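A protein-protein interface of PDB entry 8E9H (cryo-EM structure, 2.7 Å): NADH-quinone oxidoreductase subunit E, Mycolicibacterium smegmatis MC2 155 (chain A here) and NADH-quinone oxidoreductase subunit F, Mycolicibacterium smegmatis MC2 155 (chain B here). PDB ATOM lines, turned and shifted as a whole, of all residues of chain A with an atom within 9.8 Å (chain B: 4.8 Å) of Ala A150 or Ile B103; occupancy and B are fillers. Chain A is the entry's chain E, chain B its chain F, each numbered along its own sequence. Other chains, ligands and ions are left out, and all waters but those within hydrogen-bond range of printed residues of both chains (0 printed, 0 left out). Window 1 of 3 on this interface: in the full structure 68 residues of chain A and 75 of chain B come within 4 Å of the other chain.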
ATOM      1  N   CYS A 107      32.442 -16.819 -35.011  1.00  0.00           N
ATOM      2  CA  CYS A 107      31.164 -17.305 -35.510  1.00  0.00           C
ATOM      3  C   CYS A 107      31.025 -16.950 -36.980  1.00  0.00           C
ATOM      4  O   CYS A 107      30.825 -15.782 -37.326  1.00  0.00           O
ATOM      5  CB  CYS A 107      30.012 -16.709 -34.715  1.00  0.00           C
ATOM      6  SG  CYS A 107      28.408 -17.220 -35.339  1.00  0.00           S
ATOM      7  N   ASN A 109      28.664 -18.318 -39.075  1.00  0.00           N
ATOM      8  CA  ASN A 109      27.370 -18.662 -39.630  1.00  0.00           C
ATOM      9  C   ASN A 109      26.867 -17.515 -40.500  1.00  0.00           C
ATOM     10  O   ASN A 109      27.368 -16.392 -40.435  1.00  0.00           O
ATOM     11  CB  ASN A 109      26.368 -18.964 -38.521  1.00  0.00           C
ATOM     12  CG  ASN A 109      25.120 -19.631 -39.037  1.00  0.00           C
ATOM     13  OD1 ASN A 109      24.199 -18.967 -39.506  1.00  0.00           O
ATOM     14  ND2 ASN A 109      25.079 -20.953 -38.952  1.00  0.00           N
ATOM     15  N   LEU A 111      24.595 -15.218 -40.747  1.00  0.00           N
ATOM     16  CA  LEU A 111      24.432 -13.861 -40.245  1.00  0.00           C
ATOM     17  C   LEU A 111      25.770 -13.277 -39.811  1.00  0.00           C
ATOM     18  O   LEU A 111      26.287 -12.346 -40.437  1.00  0.00           O
ATOM     19  CB  LEU A 111      23.434 -13.857 -39.090  1.00  0.00           C
ATOM     20  CG  LEU A 111      22.992 -12.477 -38.618  1.00  0.00           C
ATOM     21  CD1 LEU A 111      21.542 -12.513 -38.181  1.00  0.00           C
ATOM     22  CD2 LEU A 111      23.875 -11.994 -37.487  1.00  0.00           C
ATOM     23  N   CYS A 112      26.365 -13.839 -38.759  1.00  0.00           N
ATOM     24  CA  CYS A 112      27.620 -13.295 -38.257  1.00  0.00           C
ATOM     25  C   CYS A 112      28.687 -13.296 -39.341  1.00  0.00           C
ATOM     26  O   CYS A 112      29.573 -12.437 -39.350  1.00  0.00           O
ATOM     27  CB  CYS A 112      28.088 -14.089 -37.041  1.00  0.00           C
ATOM     28  SG  CYS A 112      27.245 -13.642 -35.517  1.00  0.00           S
ATOM     29  N   VAL A 146      33.168 -21.180 -35.742  1.00  0.00           N
ATOM     30  CA  VAL A 146      32.059 -21.773 -35.012  1.00  0.00           C
ATOM     31  C   VAL A 146      30.765 -21.412 -35.720  1.00  0.00           C
ATOM     32  O   VAL A 146      30.675 -20.371 -36.376  1.00  0.00           O
ATOM     33  CB  VAL A 146      32.040 -21.289 -33.549  1.00  0.00           C
ATOM     34  CG1 VAL A 146      30.797 -21.777 -32.838  1.00  0.00           C
ATOM     35  CG2 VAL A 146      33.285 -21.760 -32.832  1.00  0.00           C
ATOM     36  N   GLU A 147      29.769 -22.280 -35.596  1.00  0.00           N
ATOM     37  CA  GLU A 147      28.458 -22.019 -36.169  1.00  0.00           C
ATOM     38  C   GLU A 147      27.740 -21.003 -35.288  1.00  0.00           C
ATOM     39  O   GLU A 147      28.311 -20.439 -34.351  1.00  0.00           O
ATOM     40  CB  GLU A 147      27.681 -23.322 -36.313  1.00  0.00           C
ATOM     41  CG  GLU A 147      28.302 -24.299 -37.295  1.00  0.00           C
ATOM     42  CD  GLU A 147      28.521 -23.696 -38.667  1.00  0.00           C
ATOM     43  OE1 GLU A 147      27.776 -22.765 -39.034  1.00  0.00           O
ATOM     44  OE2 GLU A 147      29.442 -24.149 -39.377  1.00  0.00           O
ATOM     45  N   CYS A 148      26.468 -20.752 -35.579  1.00  0.00           N
ATOM     46  CA  CYS A 148      25.727 -19.752 -34.825  1.00  0.00           C
ATOM     47  C   CYS A 148      25.800 -20.061 -33.342  1.00  0.00           C
ATOM     48  O   CYS A 148      25.597 -21.205 -32.926  1.00  0.00           O
ATOM     49  CB  CYS A 148      24.275 -19.707 -35.283  1.00  0.00           C
ATOM     50  SG  CYS A 148      23.247 -18.653 -34.249  1.00  0.00           S
ATOM     51  N   ASN A 149      26.098 -19.041 -32.543  1.00  0.00           N
ATOM     52  CA  ASN A 149      26.274 -19.198 -31.108  1.00  0.00           C
ATOM     53  C   ASN A 149      25.183 -18.487 -30.316  1.00  0.00           C
ATOM     54  O   ASN A 149      25.393 -18.109 -29.163  1.00  0.00           O
ATOM     55  CB  ASN A 149      27.644 -18.686 -30.680  1.00  0.00           C
ATOM     56  CG  ASN A 149      28.145 -19.368 -29.436  1.00  0.00           C
ATOM     57  OD1 ASN A 149      27.835 -20.528 -29.185  1.00  0.00           O
ATOM     58  ND2 ASN A 149      28.902 -18.643 -28.633  1.00  0.00           N
ATOM     59  N   ALA A 150      24.018 -18.293 -30.924  1.00  0.00           N
ATOM     60  CA  ALA A 150      22.885 -17.678 -30.243  1.00  0.00           C
ATOM     61  C   ALA A 150      23.252 -16.300 -29.701  1.00  0.00           C
ATOM     62  O   ALA A 150      22.816 -15.897 -28.622  1.00  0.00           O
ATOM     63  CB  ALA A 150      22.368 -18.580 -29.125  1.00  0.00           C
ATOM     64  N   ALA A 151      24.065 -15.575 -30.457  1.00  0.00           N
ATOM     65  CA  ALA A 151      24.408 -14.190 -30.168  1.00  0.00           C
ATOM     66  C   ALA A 151      24.284 -13.361 -31.430  1.00  0.00           C
ATOM     67  O   ALA A 151      25.055 -12.428 -31.668  1.00  0.00           O
ATOM     68  CB  ALA A 151      25.812 -14.082 -29.584  1.00  0.00           C
ATOM     69  N   CYS A 152      23.300 -13.697 -32.264  1.00  0.00           N
ATOM     70  CA  CYS A 152      23.183 -13.067 -33.571  1.00  0.00           C
ATOM     71  C   CYS A 152      22.996 -11.564 -33.458  1.00  0.00           C
ATOM     72  O   CYS A 152      23.674 -10.803 -34.155  1.00  0.00           O
ATOM     73  CB  CYS A 152      22.015 -13.682 -34.332  1.00  0.00           C
ATOM     74  SG  CYS A 152      22.224 -15.431 -34.667  1.00  0.00           S
ATOM     75  N   ASP A 153      22.092 -11.117 -32.583  1.00  0.00           N
ATOM     76  CA  ASP A 153      21.905  -9.684 -32.393  1.00  0.00           C
ATOM     77  C   ASP A 153      23.227  -9.008 -32.065  1.00  0.00           C
ATOM     78  O   ASP A 153      23.460  -7.859 -32.455  1.00  0.00           O
ATOM     79  CB  ASP A 153      20.885  -9.438 -31.285  1.00  0.00           C
ATOM     80  CG  ASP A 153      21.204 -10.207 -30.026  1.00  0.00           C
ATOM     81  OD1 ASP A 153      22.068 -11.103 -30.087  1.00  0.00           O
ATOM     82  OD2 ASP A 153      20.595  -9.921 -28.976  1.00  0.00           O
ATOM     83  N   TYR A 154      24.098  -9.691 -31.335  1.00  0.00           N
ATOM     84  CA  TYR A 154      25.445  -9.115 -31.111  1.00  0.00           C
ATOM     85  C   TYR A 154      26.269  -9.536 -32.319  1.00  0.00           C
ATOM     86  O   TYR A 154      26.939 -10.564 -32.234  1.00  0.00           O
ATOM     87  CB  TYR A 154      26.003  -9.542 -29.758  1.00  0.00           C
ATOM     88  CG  TYR A 154      25.272  -8.967 -28.574  1.00  0.00           C
ATOM     89  CD1 TYR A 154      25.566  -7.701 -28.104  1.00  0.00           C
ATOM     90  CD2 TYR A 154      24.285  -9.686 -27.924  1.00  0.00           C
ATOM     91  CE1 TYR A 154      24.901  -7.162 -27.016  1.00  0.00           C
ATOM     92  CE2 TYR A 154      23.609  -9.163 -26.835  1.00  0.00           C
ATOM     93  CZ  TYR A 154      23.918  -7.896 -26.379  1.00  0.00           C
ATOM     94  OH  TYR A 154      23.257  -7.365 -25.310  1.00  0.00           O
ATOM     95  N   ALA A 155      26.187  -8.776 -33.401  1.00  0.00           N
ATOM     96  CA  ALA A 155      26.858  -9.078 -34.685  1.00  0.00           C
ATOM     97  C   ALA A 155      28.281  -9.582 -34.538  1.00  0.00           C
ATOM     98  O   ALA A 155      28.773  -9.635 -33.416  1.00  0.00           O
ATOM     99  CB  ALA A 155      26.848  -7.804 -35.478  1.00  0.00           C
ATOM    100  N   VAL A 157      29.952 -11.754 -33.574  1.00  0.00           N
ATOM    101  CA  VAL A 157      30.344 -12.278 -32.272  1.00  0.00           C
ATOM    102  C   VAL A 157      31.577 -13.157 -32.422  1.00  0.00           C
ATOM    103  O   VAL A 157      31.768 -13.819 -33.450  1.00  0.00           O
ATOM    104  CB  VAL A 157      29.186 -13.070 -31.642  1.00  0.00           C
ATOM    105  CG1 VAL A 157      28.928 -14.332 -32.433  1.00  0.00           C
ATOM    106  CG2 VAL A 157      29.505 -13.412 -30.202  1.00  0.00           C
ATOM    107  N   MET A 159      33.796 -16.000 -29.929  1.00  0.00           N
ATOM    108  CA  MET A 159      33.853 -16.736 -28.677  1.00  0.00           C
ATOM    109  C   MET A 159      35.304 -16.941 -28.277  1.00  0.00           C
ATOM    110  O   MET A 159      36.153 -17.228 -29.121  1.00  0.00           O
ATOM    111  CB  MET A 159      33.159 -18.087 -28.815  1.00  0.00           C
ATOM    112  CG  MET A 159      31.740 -18.001 -29.328  1.00  0.00           C
ATOM    113  SD  MET A 159      30.734 -16.815 -28.425  1.00  0.00           S
ATOM    114  CE  MET A 159      30.934 -17.411 -26.752  1.00  0.00           C
ATOM    115  N   TRP A 162      34.333 -20.037 -25.249  1.00  0.00           N
ATOM    116  CA  TRP A 162      32.884 -19.946 -25.115  1.00  0.00           C
ATOM    117  C   TRP A 162      32.455 -18.764 -24.258  1.00  0.00           C
ATOM    118  O   TRP A 162      31.415 -18.818 -23.600  1.00  0.00           O
ATOM    119  CB  TRP A 162      32.310 -21.252 -24.563  1.00  0.00           C
ATOM    120  CG  TRP A 162      32.888 -22.438 -25.249  1.00  0.00           C
ATOM    121  CD1 TRP A 162      33.553 -23.477 -24.673  1.00  0.00           C
ATOM    122  CD2 TRP A 162      32.885 -22.695 -26.656  1.00  0.00           C
ATOM    123  NE1 TRP A 162      33.954 -24.372 -25.633  1.00  0.00           N
ATOM    124  CE2 TRP A 162      33.554 -23.913 -26.860  1.00  0.00           C
ATOM    125  CE3 TRP A 162      32.375 -22.014 -27.762  1.00  0.00           C
ATOM    126  CZ2 TRP A 162      33.725 -24.465 -28.122  1.00  0.00           C
ATOM    127  CZ3 TRP A 162      32.545 -22.564 -29.014  1.00  0.00           C
ATOM    128  CH2 TRP A 162      33.215 -23.776 -29.185  1.00  0.00           C
ATOM    129  N   GLU A 163      33.244 -17.695 -24.260  1.00  0.00           N
ATOM    130  CA  GLU A 163      32.867 -16.424 -23.659  1.00  0.00           C
ATOM    131  C   GLU A 163      32.671 -15.396 -24.763  1.00  0.00           C
ATOM    132  O   GLU A 163      33.504 -15.277 -25.663  1.00  0.00           O
ATOM    133  CB  GLU A 163      33.937 -15.947 -22.679  1.00  0.00           C
ATOM    134  CG  GLU A 163      34.273 -16.950 -21.596  1.00  0.00           C
ATOM    135  CD  GLU A 163      33.212 -17.027 -20.524  1.00  0.00           C
ATOM    136  OE1 GLU A 163      32.595 -15.987 -20.222  1.00  0.00           O
ATOM    137  OE2 GLU A 163      32.998 -18.128 -19.975  1.00  0.00           O
ATOM    138  N   PHE A 164      31.563 -14.665 -24.695  1.00  0.00           N
ATOM    139  CA  PHE A 164      31.163 -13.788 -25.787  1.00  0.00           C
ATOM    140  C   PHE A 164      32.082 -12.580 -25.907  1.00  0.00           C
ATOM    141  O   PHE A 164      32.580 -12.058 -24.907  1.00  0.00           O
ATOM    142  CB  PHE A 164      29.725 -13.321 -25.589  1.00  0.00           C
ATOM    143  CG  PHE A 164      28.725 -14.435 -25.574  1.00  0.00           C
ATOM    144  CD1 PHE A 164      28.283 -14.994 -26.756  1.00  0.00           C
ATOM    145  CD2 PHE A 164      28.226 -14.919 -24.382  1.00  0.00           C
ATOM    146  CE1 PHE A 164      27.362 -16.016 -26.749  1.00  0.00           C
ATOM    147  CE2 PHE A 164      27.303 -15.942 -24.370  1.00  0.00           C
ATOM    148  CZ  PHE A 164      26.872 -16.490 -25.555  1.00  0.00           C
ATOM    149  N   ASP A 166      31.247  -9.338 -28.285  1.00  0.00           N
ATOM    150  CA  ASP A 166      30.219  -8.901 -29.210  1.00  0.00           C
ATOM    151  C   ASP A 166      30.729  -7.804 -30.137  1.00  0.00           C
ATOM    152  O   ASP A 166      31.688  -7.089 -29.839  1.00  0.00           O
ATOM    153  CB  ASP A 166      29.002  -8.399 -28.440  1.00  0.00           C
ATOM    154  CG  ASP A 166      28.426  -9.450 -27.521  1.00  0.00           C
ATOM    155  OD1 ASP A 166      28.704 -10.645 -27.743  1.00  0.00           O
ATOM    156  OD2 ASP A 166      27.693  -9.085 -26.579  1.00  0.00           O
ATOM    157  N   ARG A 190      30.441 -10.117 -22.741  1.00  0.00           N
ATOM    158  CA  ARG A 190      29.299 -10.678 -22.033  1.00  0.00           C
ATOM    159  C   ARG A 190      29.682 -11.994 -21.369  1.00  0.00           C
ATOM    160  O   ARG A 190      28.946 -12.984 -21.446  1.00  0.00           O
ATOM    161  CB  ARG A 190      28.108 -10.870 -22.973  1.00  0.00           C
ATOM    162  CG  ARG A 190      26.766 -10.759 -22.287  1.00  0.00           C
ATOM    163  CD  ARG A 190      25.647 -10.457 -23.269  1.00  0.00           C
ATOM    164  NE  ARG A 190      25.232 -11.639 -24.012  1.00  0.00           N
ATOM    165  CZ  ARG A 190      25.766 -12.033 -25.160  1.00  0.00           C
ATOM    166  NH1 ARG A 190      26.739 -11.352 -25.742  1.00  0.00           N
ATOM    167  NH2 ARG A 190      25.311 -13.138 -25.741  1.00  0.00           N
ATOM    168  N   GLY A 214      28.741 -10.896 -17.518  1.00  0.00           N
ATOM    169  CA  GLY A 214      27.401 -11.294 -17.891  1.00  0.00           C
ATOM    170  C   GLY A 214      26.387 -10.176 -17.882  1.00  0.00           C
ATOM    171  O   GLY A 214      25.191 -10.441 -17.744  1.00  0.00           O
ATOM    172  N   ALA A 215      26.827  -8.930 -18.021  1.00  0.00           N
ATOM    173  CA  ALA A 215      25.891  -7.822 -18.074  1.00  0.00           C
ATOM    174  C   ALA A 215      25.005  -7.957 -19.311  1.00  0.00           C
ATOM    175  O   ALA A 215      25.437  -8.493 -20.336  1.00  0.00           O
ATOM    176  CB  ALA A 215      26.637  -6.491 -18.105  1.00  0.00           C
ATOM    177  N   PRO A 216      23.759  -7.481 -19.248  1.00  0.00           N
ATOM    178  CA  PRO A 216      22.846  -7.712 -20.380  1.00  0.00           C
ATOM    179  C   PRO A 216      23.381  -7.204 -21.705  1.00  0.00           C
ATOM    180  O   PRO A 216      23.181  -7.856 -22.737  1.00  0.00           O
ATOM    181  CB  PRO A 216      21.574  -6.966 -19.957  1.00  0.00           C
ATOM    182  CG  PRO A 216      21.651  -6.890 -18.478  1.00  0.00           C
ATOM    183  CD  PRO A 216      23.101  -6.748 -18.155  1.00  0.00           C
ATOM    184  N   ALA A 219      22.314  -4.946 -26.985  1.00  0.00           N
ATOM    185  CA  ALA A 219      21.334  -5.620 -27.830  1.00  0.00           C
ATOM    186  C   ALA A 219      20.223  -6.248 -27.001  1.00  0.00           C
ATOM    187  O   ALA A 219      19.041  -6.112 -27.334  1.00  0.00           O
ATOM    188  CB  ALA A 219      22.020  -6.679 -28.688  1.00  0.00           C
ATOM    189  N   THR A 220      20.576  -6.934 -25.915  1.00  0.00           N
ATOM    190  CA  THR A 220      19.555  -7.573 -25.094  1.00  0.00           C
ATOM    191  C   THR A 220      18.593  -6.544 -24.522  1.00  0.00           C
ATOM    192  O   THR A 220      17.424  -6.851 -24.263  1.00  0.00           O
ATOM    193  CB  THR A 220      20.203  -8.372 -23.967  1.00  0.00           C
ATOM    194  OG1 THR A 220      20.907  -7.480 -23.096  1.00  0.00           O
ATOM    195  CG2 THR A 220      21.171  -9.393 -24.527  1.00  0.00           C
ATOM    196  N   ALA B  92      17.211 -26.095 -23.145  1.00  0.00           N
ATOM    197  CA  ALA B  92      18.027 -24.892 -23.106  1.00  0.00           C
ATOM    198  C   ALA B  92      18.983 -24.810 -24.270  1.00  0.00           C
ATOM    199  O   ALA B  92      19.677 -23.800 -24.423  1.00  0.00           O
ATOM    200  CB  ALA B  92      18.795 -24.811 -21.785  1.00  0.00           C
ATOM    201  N   GLU B  94      19.965 -23.770 -27.689  1.00  0.00           N
ATOM    202  CA  GLU B  94      19.503 -22.748 -28.625  1.00  0.00           C
ATOM    203  C   GLU B  94      20.613 -22.592 -29.662  1.00  0.00           C
ATOM    204  O   GLU B  94      21.535 -21.795 -29.487  1.00  0.00           O
ATOM    205  CB  GLU B  94      19.195 -21.435 -27.922  1.00  0.00           C
ATOM    206  N   THR B  99      18.588 -17.647 -34.045  1.00  0.00           N
ATOM    207  CA  THR B  99      17.889 -17.721 -32.770  1.00  0.00           C
ATOM    208  C   THR B  99      18.831 -17.346 -31.638  1.00  0.00           C
ATOM    209  O   THR B  99      19.745 -18.105 -31.303  1.00  0.00           O
ATOM    210  CB  THR B  99      17.334 -19.123 -32.554  1.00  0.00           C
ATOM    211  OG1 THR B  99      16.665 -19.563 -33.739  1.00  0.00           O
ATOM    212  CG2 THR B  99      16.364 -19.135 -31.391  1.00  0.00           C
ATOM    213  N   CYS B 100      18.607 -16.174 -31.046  1.00  0.00           N
ATOM    214  CA  CYS B 100      19.414 -15.724 -29.922  1.00  0.00           C
ATOM    215  C   CYS B 100      18.516 -15.128 -28.847  1.00  0.00           C
ATOM    216  O   CYS B 100      18.861 -14.125 -28.216  1.00  0.00           O
ATOM    217  CB  CYS B 100      20.470 -14.710 -30.364  1.00  0.00           C
ATOM    218  SG  CYS B 100      19.828 -13.346 -31.345  1.00  0.00           S
ATOM    219  N   LYS B 101      17.351 -15.736 -28.633  1.00  0.00           N
ATOM    220  CA  LYS B 101      16.417 -15.266 -27.619  1.00  0.00           C
ATOM    221  C   LYS B 101      16.593 -16.018 -26.306  1.00  0.00           C
ATOM    222  O   LYS B 101      16.534 -15.417 -25.230  1.00  0.00           O
ATOM    223  CB  LYS B 101      14.977 -15.415 -28.114  1.00  0.00           C
ATOM    224  CG  LYS B 101      14.631 -16.799 -28.626  1.00  0.00           C
ATOM    225  CD  LYS B 101      13.155 -16.921 -28.945  1.00  0.00           C
ATOM    226  CE  LYS B 101      12.759 -18.370 -29.155  1.00  0.00           C
ATOM    227  NZ  LYS B 101      12.633 -19.101 -27.871  1.00  0.00           N
ATOM    228  N   ASP B 102      16.815 -17.328 -26.381  1.00  0.00           N
ATOM    229  CA  ASP B 102      16.960 -18.128 -25.172  1.00  0.00           C
ATOM    230  C   ASP B 102      18.165 -17.677 -24.359  1.00  0.00           C
ATOM    231  O   ASP B 102      18.090 -17.526 -23.135  1.00  0.00           O
ATOM    232  CB  ASP B 102      17.093 -19.604 -25.549  1.00  0.00           C
ATOM    233  CG  ASP B 102      15.843 -20.156 -26.197  1.00  0.00           C
ATOM    234  OD1 ASP B 102      14.744 -19.643 -25.903  1.00  0.00           O
ATOM    235  OD2 ASP B 102      15.958 -21.105 -26.999  1.00  0.00           O
ATOM    236  N   ILE B 103      19.294 -17.465 -25.031  1.00  0.00           N
ATOM    237  CA  ILE B 103      20.540 -17.192 -24.320  1.00  0.00           C
ATOM    238  C   ILE B 103      20.469 -15.886 -23.538  1.00  0.00           C
ATOM    239  O   ILE B 103      20.859 -15.877 -22.363  1.00  0.00           O
ATOM    240  CB  ILE B 103      21.725 -17.247 -25.294  1.00  0.00           C
ATOM    241  CG1 ILE B 103      21.813 -18.637 -25.930  1.00  0.00           C
ATOM    242  CG2 ILE B 103      23.045 -16.892 -24.613  1.00  0.00           C
ATOM    243  CD1 ILE B 103      21.834 -19.795 -24.946  1.00  0.00           C
ATOM    244  N   PRO B 104      20.029 -14.765 -24.112  1.00  0.00           N
ATOM    245  CA  PRO B 104      19.894 -13.550 -23.292  1.00  0.00           C
ATOM    246  C   PRO B 104      18.961 -13.738 -22.112  1.00  0.00           C
ATOM    247  O   PRO B 104      19.242 -13.247 -21.011  1.00  0.00           O
ATOM    248  CB  PRO B 104      19.357 -12.522 -24.292  1.00  0.00           C
ATOM    249  CG  PRO B 104      19.819 -13.010 -25.609  1.00  0.00           C
ATOM    250  CD  PRO B 104      19.748 -14.496 -25.530  1.00  0.00           C
ATOM    251  N   LEU B 105      17.854 -14.451 -22.313  1.00  0.00           N
ATOM    252  CA  LEU B 105      16.916 -14.666 -21.220  1.00  0.00           C
ATOM    253  C   LEU B 105      17.576 -15.430 -20.083  1.00  0.00           C
ATOM    254  O   LEU B 105      17.480 -15.031 -18.918  1.00  0.00           O
ATOM    255  CB  LEU B 105      15.689 -15.417 -21.727  1.00  0.00           C
ATOM    256  CG  LEU B 105      14.753 -15.966 -20.654  1.00  0.00           C
ATOM    257  CD1 LEU B 105      14.250 -14.845 -19.773  1.00  0.00           C
ATOM    258  CD2 LEU B 105      13.596 -16.699 -21.296  1.00  0.00           C
ATOM    259  N   LEU B 106      18.252 -16.531 -20.401  1.00  0.00           N
ATOM    260  CA  LEU B 106      18.917 -17.298 -19.357  1.00  0.00           C
ATOM    261  C   LEU B 106      20.022 -16.493 -18.699  1.00  0.00           C
ATOM    262  O   LEU B 106      20.206 -16.575 -17.480  1.00  0.00           O
ATOM    263  CB  LEU B 106      19.482 -18.591 -19.934  1.00  0.00           C
ATOM    264  CG  LEU B 106      18.446 -19.492 -20.598  1.00  0.00           C
ATOM    265  CD1 LEU B 106      19.126 -20.572 -21.416  1.00  0.00           C
ATOM    266  CD2 LEU B 106      17.533 -20.100 -19.562  1.00  0.00           C
ATOM    267  N   LEU B 107      20.767 -15.714 -19.480  1.00  0.00           N
ATOM    268  CA  LEU B 107      21.876 -14.956 -18.920  1.00  0.00           C
ATOM    269  C   LEU B 107      21.378 -13.891 -17.953  1.00  0.00           C
ATOM    270  O   LEU B 107      22.001 -13.645 -16.914  1.00  0.00           O
ATOM    271  CB  LEU B 107      22.687 -14.324 -20.046  1.00  0.00           C
ATOM    272  CG  LEU B 107      24.036 -13.761 -19.613  1.00  0.00           C
ATOM    273  CD1 LEU B 107      25.067 -14.869 -19.564  1.00  0.00           C
ATOM    274  CD2 LEU B 107      24.477 -12.655 -20.545  1.00  0.00           C
ATOM    275  N   ARG B 134      23.270 -25.847 -24.289  1.00  0.00           N
ATOM    276  CA  ARG B 134      24.413 -26.053 -25.164  1.00  0.00           C
ATOM    277  C   ARG B 134      25.691 -25.580 -24.486  1.00  0.00           C
ATOM    278  O   ARG B 134      25.681 -24.671 -23.655  1.00  0.00           O
ATOM    279  CB  ARG B 134      24.202 -25.315 -26.484  1.00  0.00           C
ATOM    280  CG  ARG B 134      24.294 -23.810 -26.371  1.00  0.00           C
ATOM    281  CD  ARG B 134      23.962 -23.136 -27.684  1.00  0.00           C
ATOM    282  NE  ARG B 134      25.001 -23.343 -28.685  1.00  0.00           N
ATOM    283  CZ  ARG B 134      25.061 -22.696 -29.840  1.00  0.00           C
ATOM    284  NH1 ARG B 134      24.161 -21.785 -30.169  1.00  0.00           N
ATOM    285  NH2 ARG B 134      26.049 -22.968 -30.686  1.00  0.00           N
ATOM    286  N   VAL B 137      27.716 -21.708 -24.714  1.00  0.00           N
ATOM    287  CA  VAL B 137      27.189 -20.498 -24.093  1.00  0.00           C
ATOM    288  C   VAL B 137      27.621 -20.467 -22.636  1.00  0.00           C
ATOM    289  O   VAL B 137      26.856 -20.054 -21.758  1.00  0.00           O
ATOM    290  CB  VAL B 137      25.662 -20.416 -24.229  1.00  0.00           C
ATOM    291  CG1 VAL B 137      25.288 -20.255 -25.685  1.00  0.00           C
ATOM    292  CG2 VAL B 137      25.008 -21.648 -23.644  1.00  0.00           C
ATOM    293  N   VAL B 140      26.023 -18.527 -19.957  1.00  0.00           N
ATOM    294  CA  VAL B 140      24.665 -18.922 -19.607  1.00  0.00           C
ATOM    295  C   VAL B 140      24.693 -20.158 -18.726  1.00  0.00           C
ATOM    296  O   VAL B 140      23.871 -20.310 -17.820  1.00  0.00           O
ATOM    297  CB  VAL B 140      23.826 -19.151 -20.875  1.00  0.00           C
ATOM    298  CG1 VAL B 140      22.603 -19.998 -20.557  1.00  0.00           C
ATOM    299  CG2 VAL B 140      23.412 -17.823 -21.470  1.00  0.00           C
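The backbone carbonyl oxygen (O) of Cys A148 sits at hydrogen-bond distance from the guanidinium group (NH2) of Arg B134. OD1 of Asn A149 lies within hydrogen-bond range of NH2 of Arg B134, at 3.4 Å. N of Cys A152 sits close to SG of Cys B100, at 3.6 Å. N of Asp A153 is in hydrogen-bond range of SG of Cys B100, at 3.4 Å.
The side-chain sulfur (SG) of Cys A148 lies close to the backbone NH (N) of Ala A150, 3.4 Å away. The side-chain sulfur of Met A159 is in hydrogen-bond range of the side-chain amide nitrogen of Asn A149 (2.6 Å). The backbone NH (N) of Thr A220 lies within hydrogen-bond range of the side-chain hydroxyl (OH) of Tyr A154, at 2.8 Å. NH1 of Arg A190 lies within salt-bridge range of OD2 of Asp A166. The backbone carbonyl oxygen of Glu B94 lies within hydrogen-bond range of the guanidinium group of Arg B134 (2.7 Å).
Ala A150 touches Glu B94 (CB to O, 3.3 Å). Ala A150 touches Thr B99 (CA to O, 3.3 Å). Cys B100 touches Ala A150 (CB to O, 3.2 Å). Ala A150 touches Ile B103 (CB to CG1, 3.2 Å). N of Ala A150 touches NH1 of Arg B134, at 3.6 Å. Ala A151 touches Cys B100. Phe A164 touches Ile B103 (CZ to CG2, 3.96 Å). CG of Arg A190 touches CD2 of Leu B107, at 3.4 Å. O of Gly A214 touches CD2 of Leu B107 (3.6 Å). CB of Pro B104 touches CG2 of Thr A220, at 3.6 Å.
Of chain B, only Glu B94, Thr B99, Cys B100, Ile B103 and Arg B134 come within 4 Å of Ala A150. Of the printed residues of chain B, Ala A151 touches Cys B100 (3.7 Å). Of chain A, only Ala A150 (3.3 Å) comes within 4 Å of Glu B94. Of the printed residues of chain A, Thr B99 touches Ala A150 (3.3 Å). Of chain A, only Ala A150, Ala A151, Cys A152 and Asp A153 come within 4 Å of Cys B100. Of chain A, only Ala A150 (3.2 Å) and Phe A164 (3.96 Å) come within 4 Å of Ile B103. Of the printed residues of chain A, Pro B104 touches Thr A220 (3.6 Å). Printed residues of chain A within 4 Å of Arg B134: Cys A148 (2.9 Å), Asn A149 (3.4 Å) and Ala A150 (3.6 Å). The nearest residue of chain B that does not touch Ala A150 is Pro B104 (4.6 Å). The nearest printed residue of chain B that does not touch Ala A151 is Thr B99 (5.1 Å).
Hydrophobic or aromatic side chains of chain B that line the printed part of chain A: Ile B103, Pro B104 and Leu B107. Along chain B the printed residues that touch a printed residue of chain A span positions 94 to 134. Hydrophobic or aromatic side chains of chain A that line the printed part of chain B: Ala A150 and Phe A164.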
